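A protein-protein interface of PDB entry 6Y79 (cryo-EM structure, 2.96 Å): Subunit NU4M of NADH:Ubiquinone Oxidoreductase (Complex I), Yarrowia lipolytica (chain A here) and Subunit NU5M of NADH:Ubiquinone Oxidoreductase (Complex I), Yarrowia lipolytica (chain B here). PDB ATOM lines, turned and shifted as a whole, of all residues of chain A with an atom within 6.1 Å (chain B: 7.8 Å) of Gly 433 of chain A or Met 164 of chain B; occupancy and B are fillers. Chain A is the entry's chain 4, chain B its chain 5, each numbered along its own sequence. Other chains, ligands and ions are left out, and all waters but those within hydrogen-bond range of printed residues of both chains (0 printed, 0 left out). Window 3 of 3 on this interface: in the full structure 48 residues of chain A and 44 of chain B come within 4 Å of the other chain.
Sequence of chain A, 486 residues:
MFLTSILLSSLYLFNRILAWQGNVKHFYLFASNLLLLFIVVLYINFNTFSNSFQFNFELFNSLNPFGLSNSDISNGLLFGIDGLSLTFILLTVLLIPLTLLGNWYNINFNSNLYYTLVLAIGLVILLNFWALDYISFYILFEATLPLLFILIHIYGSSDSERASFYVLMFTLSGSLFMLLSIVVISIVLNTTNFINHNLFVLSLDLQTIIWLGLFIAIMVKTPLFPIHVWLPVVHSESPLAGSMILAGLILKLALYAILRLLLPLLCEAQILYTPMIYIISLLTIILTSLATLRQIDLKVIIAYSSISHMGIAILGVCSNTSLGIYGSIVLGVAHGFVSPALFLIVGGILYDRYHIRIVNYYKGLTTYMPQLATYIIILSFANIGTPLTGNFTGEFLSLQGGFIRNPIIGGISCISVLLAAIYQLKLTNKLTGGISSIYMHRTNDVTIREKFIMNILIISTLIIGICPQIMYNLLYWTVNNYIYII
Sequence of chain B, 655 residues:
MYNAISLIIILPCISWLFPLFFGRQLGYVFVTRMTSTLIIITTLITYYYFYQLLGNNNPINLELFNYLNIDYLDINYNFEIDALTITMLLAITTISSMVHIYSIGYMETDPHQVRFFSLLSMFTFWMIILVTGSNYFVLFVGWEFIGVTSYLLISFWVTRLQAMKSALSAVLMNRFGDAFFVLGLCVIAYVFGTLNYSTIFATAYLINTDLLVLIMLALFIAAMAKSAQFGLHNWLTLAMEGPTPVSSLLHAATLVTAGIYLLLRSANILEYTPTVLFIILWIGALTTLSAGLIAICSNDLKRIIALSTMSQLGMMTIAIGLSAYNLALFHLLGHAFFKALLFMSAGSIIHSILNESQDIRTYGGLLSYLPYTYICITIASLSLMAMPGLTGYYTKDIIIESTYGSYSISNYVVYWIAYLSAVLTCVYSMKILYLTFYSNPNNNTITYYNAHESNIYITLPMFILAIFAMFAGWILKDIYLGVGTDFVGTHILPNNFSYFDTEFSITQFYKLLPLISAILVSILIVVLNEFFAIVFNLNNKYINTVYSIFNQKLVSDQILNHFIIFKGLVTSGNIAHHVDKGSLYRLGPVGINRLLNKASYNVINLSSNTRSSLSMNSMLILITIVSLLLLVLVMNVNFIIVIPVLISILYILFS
The backbone NH of Gly 434 of chain A sits at hydrogen-bond distance from the backbone carbonyl oxygen of Val 158 of chain B (2.5 Å).
Val 158 of chain B touches Thr 366 of chain A (CG2 to OG1, 3.5 Å). CB of Asn 429 of chain A touches OH of Tyr 151 of chain B, at 3.2 Å. Asn 429 of chain A touches Met 164 of chain B. Leu 168 of chain B touches Asn 429 of chain A (CD2 to ND2, 3.4 Å). Thr 432 of chain A touches Tyr 151 of chain B. Gly 433 of chain A touches Val 158 of chain B (C to O, 3.4 Å). CE of Met 164 of chain B touches CA of Gly 433 of chain A, 3.7 Å away. Gly 434 of chain A touches Thr 159 of chain B (O to CA, 3.8 Å). Ile 435 of chain A touches Thr 159 of chain B.
Of the printed residues of chain B, Gly 433 of chain A touches Val 158 and Met 164. Printed residues of chain A within 4 Å of Met 164 of chain B: Asn 429 (3.5 Å) and Gly 433 (3.7 Å). Gly 434 of chain A touches two residues of chain B. Of the printed residues of chain B, Thr 366 of chain A touches Val 158. Of the printed residues of chain A, Tyr 151 of chain B touches Asn 429 (3.2 Å) and Thr 432 (3.9 Å). Printed residues of chain B within 4 Å of Ile 435 of chain A: Thr 159 (3.9 Å). Of the printed residues of chain B, Asn 429 of chain A touches Tyr 151, Met 164 and Leu 168. Printed residues of chain B within 4 Å of Thr 432 of chain A: Tyr 151 (3.9 Å). The nearest residue of chain B that does not touch Gly 433 of chain A is Thr 159 of chain B (5.5 Å). The nearest printed residue of chain A that does not touch Met 164 of chain B is Thr 432 of chain A (4.01 Å).
O of Tyr 151 of chain B lies within hydrogen-bond range of OG of Ser 155 of chain B (2.5 Å). O of Thr 428 of chain A is in hydrogen-bond range of OG1 of Thr 432 of chain A (2.8 Å). N of Gly 364 of chain A is in hydrogen-bond range of O of Gly 433 of chain A.
Among the printed residues, 10 pairs touch across the chains.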
ATOM      1  N   LYS A 363      -3.757 -16.906 -34.414  1.00  0.00           N
ATOM      2  CA  LYS A 363      -3.472 -17.164 -33.012  1.00  0.00           C
ATOM      3  C   LYS A 363      -3.217 -15.834 -32.327  1.00  0.00           C
ATOM      4  O   LYS A 363      -2.518 -14.980 -32.874  1.00  0.00           O
ATOM      5  CB  LYS A 363      -2.261 -18.085 -32.848  1.00  0.00           C
ATOM      6  CG  LYS A 363      -1.981 -18.490 -31.421  1.00  0.00           C
ATOM      7  CD  LYS A 363      -0.822 -19.453 -31.328  1.00  0.00           C
ATOM      8  CE  LYS A 363       0.464 -18.770 -31.692  1.00  0.00           C
ATOM      9  NZ  LYS A 363       1.635 -19.568 -31.277  1.00  0.00           N
ATOM     10  N   GLY A 364      -3.791 -15.663 -31.141  1.00  0.00           N
ATOM     11  CA  GLY A 364      -3.495 -14.515 -30.311  1.00  0.00           C
ATOM     12  C   GLY A 364      -3.983 -13.202 -30.866  1.00  0.00           C
ATOM     13  O   GLY A 364      -3.237 -12.223 -30.908  1.00  0.00           O
ATOM     14  N   LEU A 365      -5.237 -13.166 -31.296  1.00  0.00           N
ATOM     15  CA  LEU A 365      -5.795 -11.971 -31.909  1.00  0.00           C
ATOM     16  C   LEU A 365      -6.181 -10.889 -30.904  1.00  0.00           C
ATOM     17  O   LEU A 365      -6.574  -9.806 -31.339  1.00  0.00           O
ATOM     18  CB  LEU A 365      -7.016 -12.351 -32.758  1.00  0.00           C
ATOM     19  CG  LEU A 365      -6.879 -12.744 -34.233  1.00  0.00           C
ATOM     20  CD1 LEU A 365      -6.285 -14.126 -34.399  1.00  0.00           C
ATOM     21  CD2 LEU A 365      -8.238 -12.695 -34.880  1.00  0.00           C
ATOM     22  N   THR A 366      -6.066 -11.131 -29.587  1.00  0.00           N
ATOM     23  CA  THR A 366      -6.497 -10.132 -28.605  1.00  0.00           C
ATOM     24  C   THR A 366      -5.520  -8.982 -28.494  1.00  0.00           C
ATOM     25  O   THR A 366      -5.916  -7.858 -28.174  1.00  0.00           O
ATOM     26  CB  THR A 366      -6.619 -10.710 -27.197  1.00  0.00           C
ATOM     27  OG1 THR A 366      -5.327 -11.120 -26.733  1.00  0.00           O
ATOM     28  CG2 THR A 366      -7.607 -11.859 -27.093  1.00  0.00           C
ATOM     29  N   THR A 428     -12.732 -20.605 -30.484  1.00  0.00           N
ATOM     30  CA  THR A 428     -12.650 -19.265 -29.917  1.00  0.00           C
ATOM     31  C   THR A 428     -11.399 -19.077 -29.071  1.00  0.00           C
ATOM     32  O   THR A 428     -10.762 -18.020 -29.134  1.00  0.00           O
ATOM     33  CB  THR A 428     -13.911 -18.999 -29.106  1.00  0.00           C
ATOM     34  OG1 THR A 428     -15.035 -19.162 -29.968  1.00  0.00           O
ATOM     35  CG2 THR A 428     -13.930 -17.604 -28.543  1.00  0.00           C
ATOM     36  N   ASN A 429     -11.005 -20.085 -28.289  1.00  0.00           N
ATOM     37  CA  ASN A 429      -9.807 -19.895 -27.477  1.00  0.00           C
ATOM     38  C   ASN A 429      -8.540 -19.986 -28.316  1.00  0.00           C
ATOM     39  O   ASN A 429      -7.509 -19.424 -27.939  1.00  0.00           O
ATOM     40  CB  ASN A 429      -9.770 -20.881 -26.307  1.00  0.00           C
ATOM     41  CG  ASN A 429      -9.393 -22.262 -26.711  1.00  0.00           C
ATOM     42  OD1 ASN A 429      -9.736 -22.731 -27.790  1.00  0.00           O
ATOM     43  ND2 ASN A 429      -8.672 -22.940 -25.836  1.00  0.00           N
ATOM     44  N   LYS A 430      -8.596 -20.685 -29.447  1.00  0.00           N
ATOM     45  CA  LYS A 430      -7.481 -20.672 -30.384  1.00  0.00           C
ATOM     46  C   LYS A 430      -7.338 -19.309 -31.044  1.00  0.00           C
ATOM     47  O   LYS A 430      -6.221 -18.808 -31.209  1.00  0.00           O
ATOM     48  CB  LYS A 430      -7.677 -21.759 -31.436  1.00  0.00           C
ATOM     49  CG  LYS A 430      -6.666 -21.748 -32.558  1.00  0.00           C
ATOM     50  CD  LYS A 430      -5.296 -22.128 -32.057  1.00  0.00           C
ATOM     51  CE  LYS A 430      -4.299 -22.287 -33.192  1.00  0.00           C
ATOM     52  NZ  LYS A 430      -4.513 -23.546 -33.960  1.00  0.00           N
ATOM     53  N   LEU A 431      -8.458 -18.691 -31.423  1.00  0.00           N
ATOM     54  CA  LEU A 431      -8.389 -17.384 -32.069  1.00  0.00           C
ATOM     55  C   LEU A 431      -7.982 -16.295 -31.091  1.00  0.00           C
ATOM     56  O   LEU A 431      -7.198 -15.409 -31.439  1.00  0.00           O
ATOM     57  CB  LEU A 431      -9.729 -17.025 -32.703  1.00  0.00           C
ATOM     58  CG  LEU A 431     -10.187 -17.797 -33.933  1.00  0.00           C
ATOM     59  CD1 LEU A 431     -11.551 -17.310 -34.342  1.00  0.00           C
ATOM     60  CD2 LEU A 431      -9.214 -17.621 -35.051  1.00  0.00           C
ATOM     61  N   THR A 432      -8.503 -16.333 -29.870  1.00  0.00           N
ATOM     62  CA  THR A 432      -8.217 -15.239 -28.958  1.00  0.00           C
ATOM     63  C   THR A 432      -6.913 -15.470 -28.200  1.00  0.00           C
ATOM     64  O   THR A 432      -6.106 -14.552 -28.081  1.00  0.00           O
ATOM     65  CB  THR A 432      -9.408 -15.027 -28.021  1.00  0.00           C
ATOM     66  OG1 THR A 432      -9.708 -16.236 -27.313  1.00  0.00           O
ATOM     67  CG2 THR A 432     -10.633 -14.644 -28.841  1.00  0.00           C
ATOM     68  N   GLY A 433      -6.622 -16.698 -27.778  1.00  0.00           N
ATOM     69  CA  GLY A 433      -5.493 -16.974 -26.920  1.00  0.00           C
ATOM     70  C   GLY A 433      -4.175 -17.177 -27.650  1.00  0.00           C
ATOM     71  O   GLY A 433      -4.117 -17.411 -28.853  1.00  0.00           O
ATOM     72  N   GLY A 434      -3.097 -17.079 -26.876  1.00  0.00           N
ATOM     73  CA  GLY A 434      -1.747 -17.306 -27.352  1.00  0.00           C
ATOM     74  C   GLY A 434      -0.977 -16.015 -27.596  1.00  0.00           C
ATOM     75  O   GLY A 434      -1.508 -14.904 -27.540  1.00  0.00           O
ATOM     76  N   ILE A 435       0.325 -16.181 -27.847  1.00  0.00           N
ATOM     77  CA  ILE A 435       1.123 -15.087 -28.387  1.00  0.00           C
ATOM     78  C   ILE A 435       0.620 -14.817 -29.795  1.00  0.00           C
ATOM     79  O   ILE A 435       0.125 -15.726 -30.471  1.00  0.00           O
ATOM     80  CB  ILE A 435       2.622 -15.447 -28.345  1.00  0.00           C
ATOM     81  CG1 ILE A 435       3.052 -15.740 -26.911  1.00  0.00           C
ATOM     82  CG2 ILE A 435       3.518 -14.353 -28.887  1.00  0.00           C
ATOM     83  CD1 ILE A 435       4.419 -16.360 -26.803  1.00  0.00           C
ATOM     84  N   TYR B 151     -14.483 -19.074 -17.698  1.00  0.00           N
ATOM     85  CA  TYR B 151     -13.663 -19.000 -18.906  1.00  0.00           C
ATOM     86  C   TYR B 151     -12.851 -17.720 -18.941  1.00  0.00           C
ATOM     87  O   TYR B 151     -11.629 -17.742 -19.106  1.00  0.00           O
ATOM     88  CB  TYR B 151     -14.528 -19.064 -20.159  1.00  0.00           C
ATOM     89  CG  TYR B 151     -13.754 -19.009 -21.444  1.00  0.00           C
ATOM     90  CD1 TYR B 151     -13.052 -20.105 -21.914  1.00  0.00           C
ATOM     91  CD2 TYR B 151     -13.742 -17.855 -22.197  1.00  0.00           C
ATOM     92  CE1 TYR B 151     -12.354 -20.029 -23.095  1.00  0.00           C
ATOM     93  CE2 TYR B 151     -13.057 -17.766 -23.349  1.00  0.00           C
ATOM     94  CZ  TYR B 151     -12.369 -18.845 -23.802  1.00  0.00           C
ATOM     95  OH  TYR B 151     -11.700 -18.694 -24.980  1.00  0.00           O
ATOM     96  N   ILE B 154     -10.130 -17.695 -15.789  1.00  0.00           N
ATOM     97  CA  ILE B 154      -9.004 -18.626 -15.815  1.00  0.00           C
ATOM     98  C   ILE B 154      -8.075 -18.297 -16.976  1.00  0.00           C
ATOM     99  O   ILE B 154      -6.853 -18.438 -16.872  1.00  0.00           O
ATOM    100  CB  ILE B 154      -9.535 -20.073 -15.872  1.00  0.00           C
ATOM    101  CG1 ILE B 154     -10.291 -20.409 -14.595  1.00  0.00           C
ATOM    102  CG2 ILE B 154      -8.429 -21.083 -16.018  1.00  0.00           C
ATOM    103  CD1 ILE B 154     -11.167 -21.610 -14.736  1.00  0.00           C
ATOM    104  N   SER B 155      -8.622 -17.767 -18.061  1.00  0.00           N
ATOM    105  CA  SER B 155      -7.850 -17.390 -19.237  1.00  0.00           C
ATOM    106  C   SER B 155      -7.484 -15.924 -19.225  1.00  0.00           C
ATOM    107  O   SER B 155      -7.519 -15.277 -20.273  1.00  0.00           O
ATOM    108  CB  SER B 155      -8.644 -17.725 -20.489  1.00  0.00           C
ATOM    109  OG  SER B 155      -9.798 -16.913 -20.575  1.00  0.00           O
ATOM    110  N   PHE B 156      -7.175 -15.369 -18.050  1.00  0.00           N
ATOM    111  CA  PHE B 156      -6.880 -13.944 -17.951  1.00  0.00           C
ATOM    112  C   PHE B 156      -5.582 -13.594 -18.659  1.00  0.00           C
ATOM    113  O   PHE B 156      -5.488 -12.547 -19.306  1.00  0.00           O
ATOM    114  CB  PHE B 156      -6.813 -13.514 -16.493  1.00  0.00           C
ATOM    115  CG  PHE B 156      -6.542 -12.059 -16.326  1.00  0.00           C
ATOM    116  CD1 PHE B 156      -7.500 -11.129 -16.669  1.00  0.00           C
ATOM    117  CD2 PHE B 156      -5.323 -11.615 -15.853  1.00  0.00           C
ATOM    118  CE1 PHE B 156      -7.249  -9.787 -16.535  1.00  0.00           C
ATOM    119  CE2 PHE B 156      -5.074 -10.273 -15.718  1.00  0.00           C
ATOM    120  CZ  PHE B 156      -6.037  -9.364 -16.060  1.00  0.00           C
ATOM    121  N   TRP B 157      -4.572 -14.448 -18.554  1.00  0.00           N
ATOM    122  CA  TRP B 157      -3.377 -14.303 -19.372  1.00  0.00           C
ATOM    123  C   TRP B 157      -3.606 -15.090 -20.644  1.00  0.00           C
ATOM    124  O   TRP B 157      -3.380 -16.299 -20.696  1.00  0.00           O
ATOM    125  CB  TRP B 157      -2.133 -14.744 -18.622  1.00  0.00           C
ATOM    126  CG  TRP B 157      -1.857 -13.776 -17.570  1.00  0.00           C
ATOM    127  CD1 TRP B 157      -1.438 -12.496 -17.736  1.00  0.00           C
ATOM    128  CD2 TRP B 157      -2.018 -13.970 -16.174  1.00  0.00           C
ATOM    129  NE1 TRP B 157      -1.320 -11.878 -16.523  1.00  0.00           N
ATOM    130  CE2 TRP B 157      -1.671 -12.767 -15.546  1.00  0.00           C
ATOM    131  CE3 TRP B 157      -2.413 -15.051 -15.392  1.00  0.00           C
ATOM    132  CZ2 TRP B 157      -1.708 -12.614 -14.175  1.00  0.00           C
ATOM    133  CZ3 TRP B 157      -2.446 -14.897 -14.031  1.00  0.00           C
ATOM    134  CH2 TRP B 157      -2.092 -13.690 -13.434  1.00  0.00           C
ATOM    135  N   VAL B 158      -4.080 -14.383 -21.669  1.00  0.00           N
ATOM    136  CA  VAL B 158      -4.339 -14.969 -22.968  1.00  0.00           C
ATOM    137  C   VAL B 158      -3.055 -15.395 -23.657  1.00  0.00           C
ATOM    138  O   VAL B 158      -3.086 -16.266 -24.530  1.00  0.00           O
ATOM    139  CB  VAL B 158      -5.130 -13.957 -23.808  1.00  0.00           C
ATOM    140  CG1 VAL B 158      -6.548 -13.879 -23.311  1.00  0.00           C
ATOM    141  CG2 VAL B 158      -4.494 -12.593 -23.689  1.00  0.00           C
ATOM    142  N   THR B 159      -1.922 -14.805 -23.269  1.00  0.00           N
ATOM    143  CA  THR B 159      -0.632 -15.172 -23.838  1.00  0.00           C
ATOM    144  C   THR B 159      -0.206 -16.562 -23.398  1.00  0.00           C
ATOM    145  O   THR B 159       0.488 -17.267 -24.136  1.00  0.00           O
ATOM    146  CB  THR B 159       0.415 -14.147 -23.428  1.00  0.00           C
ATOM    147  OG1 THR B 159       0.528 -14.137 -22.000  1.00  0.00           O
ATOM    148  CG2 THR B 159      -0.002 -12.771 -23.887  1.00  0.00           C
ATOM    149  N   ARG B 160      -0.607 -16.973 -22.202  1.00  0.00           N
ATOM    150  CA  ARG B 160      -0.219 -18.280 -21.697  1.00  0.00           C
ATOM    151  C   ARG B 160      -1.075 -19.365 -22.326  1.00  0.00           C
ATOM    152  O   ARG B 160      -2.300 -19.261 -22.377  1.00  0.00           O
ATOM    153  CB  ARG B 160      -0.336 -18.320 -20.181  1.00  0.00           C
ATOM    154  CG  ARG B 160       0.332 -19.519 -19.570  1.00  0.00           C
ATOM    155  CD  ARG B 160       0.326 -19.445 -18.060  1.00  0.00           C
ATOM    156  NE  ARG B 160       0.648 -20.736 -17.473  1.00  0.00           N
ATOM    157  CZ  ARG B 160       1.882 -21.171 -17.270  1.00  0.00           C
ATOM    158  NH1 ARG B 160       2.911 -20.411 -17.599  1.00  0.00           N
ATOM    159  NH2 ARG B 160       2.088 -22.362 -16.737  1.00  0.00           N
ATOM    160  N   LEU B 161      -0.415 -20.412 -22.803  1.00  0.00           N
ATOM    161  CA  LEU B 161      -1.094 -21.503 -23.487  1.00  0.00           C
ATOM    162  C   LEU B 161      -1.859 -22.389 -22.521  1.00  0.00           C
ATOM    163  O   LEU B 161      -2.999 -22.789 -22.797  1.00  0.00           O
ATOM    164  CB  LEU B 161      -0.054 -22.323 -24.208  1.00  0.00           C
ATOM    165  CG  LEU B 161      -0.417 -23.384 -25.201  1.00  0.00           C
ATOM    166  CD1 LEU B 161       0.698 -23.155 -26.054  1.00  0.00           C
ATOM    167  CD2 LEU B 161      -0.292 -24.756 -24.598  1.00  0.00           C
ATOM    168  N   GLN B 162      -1.220 -22.741 -21.407  1.00  0.00           N
ATOM    169  CA  GLN B 162      -1.826 -23.632 -20.431  1.00  0.00           C
ATOM    170  C   GLN B 162      -3.027 -22.990 -19.763  1.00  0.00           C
ATOM    171  O   GLN B 162      -3.970 -23.693 -19.400  1.00  0.00           O
ATOM    172  CB  GLN B 162      -0.786 -24.040 -19.395  1.00  0.00           C
ATOM    173  CG  GLN B 162       0.357 -24.839 -19.979  1.00  0.00           C
ATOM    174  CD  GLN B 162      -0.092 -26.186 -20.502  1.00  0.00           C
ATOM    175  OE1 GLN B 162      -0.856 -26.892 -19.849  1.00  0.00           O
ATOM    176  NE2 GLN B 162       0.377 -26.549 -21.689  1.00  0.00           N
ATOM    177  N   ALA B 163      -3.036 -21.660 -19.652  1.00  0.00           N
ATOM    178  CA  ALA B 163      -4.205 -20.962 -19.132  1.00  0.00           C
ATOM    179  C   ALA B 163      -5.384 -21.058 -20.090  1.00  0.00           C
ATOM    180  O   ALA B 163      -6.522 -21.265 -19.655  1.00  0.00           O
ATOM    181  CB  ALA B 163      -3.859 -19.502 -18.854  1.00  0.00           C
ATOM    182  N   MET B 164      -5.131 -20.928 -21.395  1.00  0.00           N
ATOM    183  CA  MET B 164      -6.200 -21.032 -22.383  1.00  0.00           C
ATOM    184  C   MET B 164      -6.781 -22.436 -22.420  1.00  0.00           C
ATOM    185  O   MET B 164      -8.008 -22.614 -22.391  1.00  0.00           O
ATOM    186  CB  MET B 164      -5.683 -20.638 -23.766  1.00  0.00           C
ATOM    187  CG  MET B 164      -5.245 -19.204 -23.895  1.00  0.00           C
ATOM    188  SD  MET B 164      -6.467 -18.025 -23.319  1.00  0.00           S
ATOM    189  CE  MET B 164      -7.828 -18.306 -24.440  1.00  0.00           C
ATOM    190  N   LYS B 165      -5.912 -23.449 -22.444  1.00  0.00           N
ATOM    191  CA  LYS B 165      -6.388 -24.829 -22.455  1.00  0.00           C
ATOM    192  C   LYS B 165      -7.048 -25.215 -21.135  1.00  0.00           C
ATOM    193  O   LYS B 165      -7.986 -26.022 -21.119  1.00  0.00           O
ATOM    194  CB  LYS B 165      -5.229 -25.759 -22.782  1.00  0.00           C
ATOM    195  CG  LYS B 165      -4.779 -25.658 -24.220  1.00  0.00           C
ATOM    196  CD  LYS B 165      -3.559 -26.496 -24.484  1.00  0.00           C
ATOM    197  CE  LYS B 165      -3.874 -27.955 -24.380  1.00  0.00           C
ATOM    198  NZ  LYS B 165      -2.668 -28.779 -24.640  1.00  0.00           N
ATOM    199  N   SER B 166      -6.636 -24.585 -20.038  1.00  0.00           N
ATOM    200  CA  SER B 166      -7.228 -24.852 -18.737  1.00  0.00           C
ATOM    201  C   SER B 166      -8.624 -24.257 -18.616  1.00  0.00           C
ATOM    202  O   SER B 166      -9.535 -24.901 -18.075  1.00  0.00           O
ATOM    203  CB  SER B 166      -6.305 -24.290 -17.670  1.00  0.00           C
ATOM    204  OG  SER B 166      -5.171 -25.115 -17.526  1.00  0.00           O
ATOM    205  N   ALA B 167      -8.811 -23.034 -19.114  1.00  0.00           N
ATOM    206  CA  ALA B 167     -10.143 -22.441 -19.152  1.00  0.00           C
ATOM    207  C   ALA B 167     -11.068 -23.220 -20.075  1.00  0.00           C
ATOM    208  O   ALA B 167     -12.262 -23.378 -19.782  1.00  0.00           O
ATOM    209  CB  ALA B 167     -10.052 -20.988 -19.592  1.00  0.00           C
ATOM    210  N   LEU B 168     -10.519 -23.744 -21.175  1.00  0.00           N
ATOM    211  CA  LEU B 168     -11.295 -24.568 -22.095  1.00  0.00           C
ATOM    212  C   LEU B 168     -11.787 -25.850 -21.426  1.00  0.00           C
ATOM    213  O   LEU B 168     -12.960 -26.221 -21.563  1.00  0.00           O
ATOM    214  CB  LEU B 168     -10.441 -24.880 -23.317  1.00  0.00           C
ATOM    215  CG  LEU B 168     -10.958 -25.783 -24.425  1.00  0.00           C
ATOM    216  CD1 LEU B 168     -12.015 -25.086 -25.219  1.00  0.00           C
ATOM    217  CD2 LEU B 168      -9.797 -26.120 -25.304  1.00  0.00           C
ATOM    218  N   SER B 169     -10.913 -26.519 -20.668  1.00  0.00           N
ATOM    219  CA  SER B 169     -11.314 -27.744 -19.980  1.00  0.00           C
ATOM    220  C   SER B 169     -12.337 -27.464 -18.883  1.00  0.00           C
ATOM    221  O   SER B 169     -13.289 -28.235 -18.702  1.00  0.00           O
ATOM    222  CB  SER B 169     -10.093 -28.455 -19.401  1.00  0.00           C
ATOM    223  OG  SER B 169      -9.519 -27.725 -18.338  1.00  0.00           O
ATOM    224  N   ALA B 170     -12.169 -26.350 -18.159  1.00  0.00           N
ATOM    225  CA  ALA B 170     -13.104 -26.008 -17.088  1.00  0.00           C
ATOM    226  C   ALA B 170     -14.501 -25.731 -17.624  1.00  0.00           C
ATOM    227  O   ALA B 170     -15.503 -26.229 -17.085  1.00  0.00           O
ATOM    228  CB  ALA B 170     -12.588 -24.801 -16.312  1.00  0.00           C
ATOM    229  N   GLU B 241      -4.087 -22.108 -13.074  1.00  0.00           N
ATOM    230  CA  GLU B 241      -3.399 -21.257 -14.030  1.00  0.00           C
ATOM    231  C   GLU B 241      -3.969 -19.850 -14.044  1.00  0.00           C
ATOM    232  O   GLU B 241      -3.271 -18.916 -14.449  1.00  0.00           O
ATOM    233  CB  GLU B 241      -3.462 -21.883 -15.423  1.00  0.00           C
ATOM    234  CG  GLU B 241      -2.637 -23.155 -15.563  1.00  0.00           C
ATOM    235  CD  GLU B 241      -3.373 -24.395 -15.091  1.00  0.00           C
ATOM    236  OE1 GLU B 241      -4.557 -24.269 -14.713  1.00  0.00           O
ATOM    237  OE2 GLU B 241      -2.779 -25.496 -15.109  1.00  0.00           O
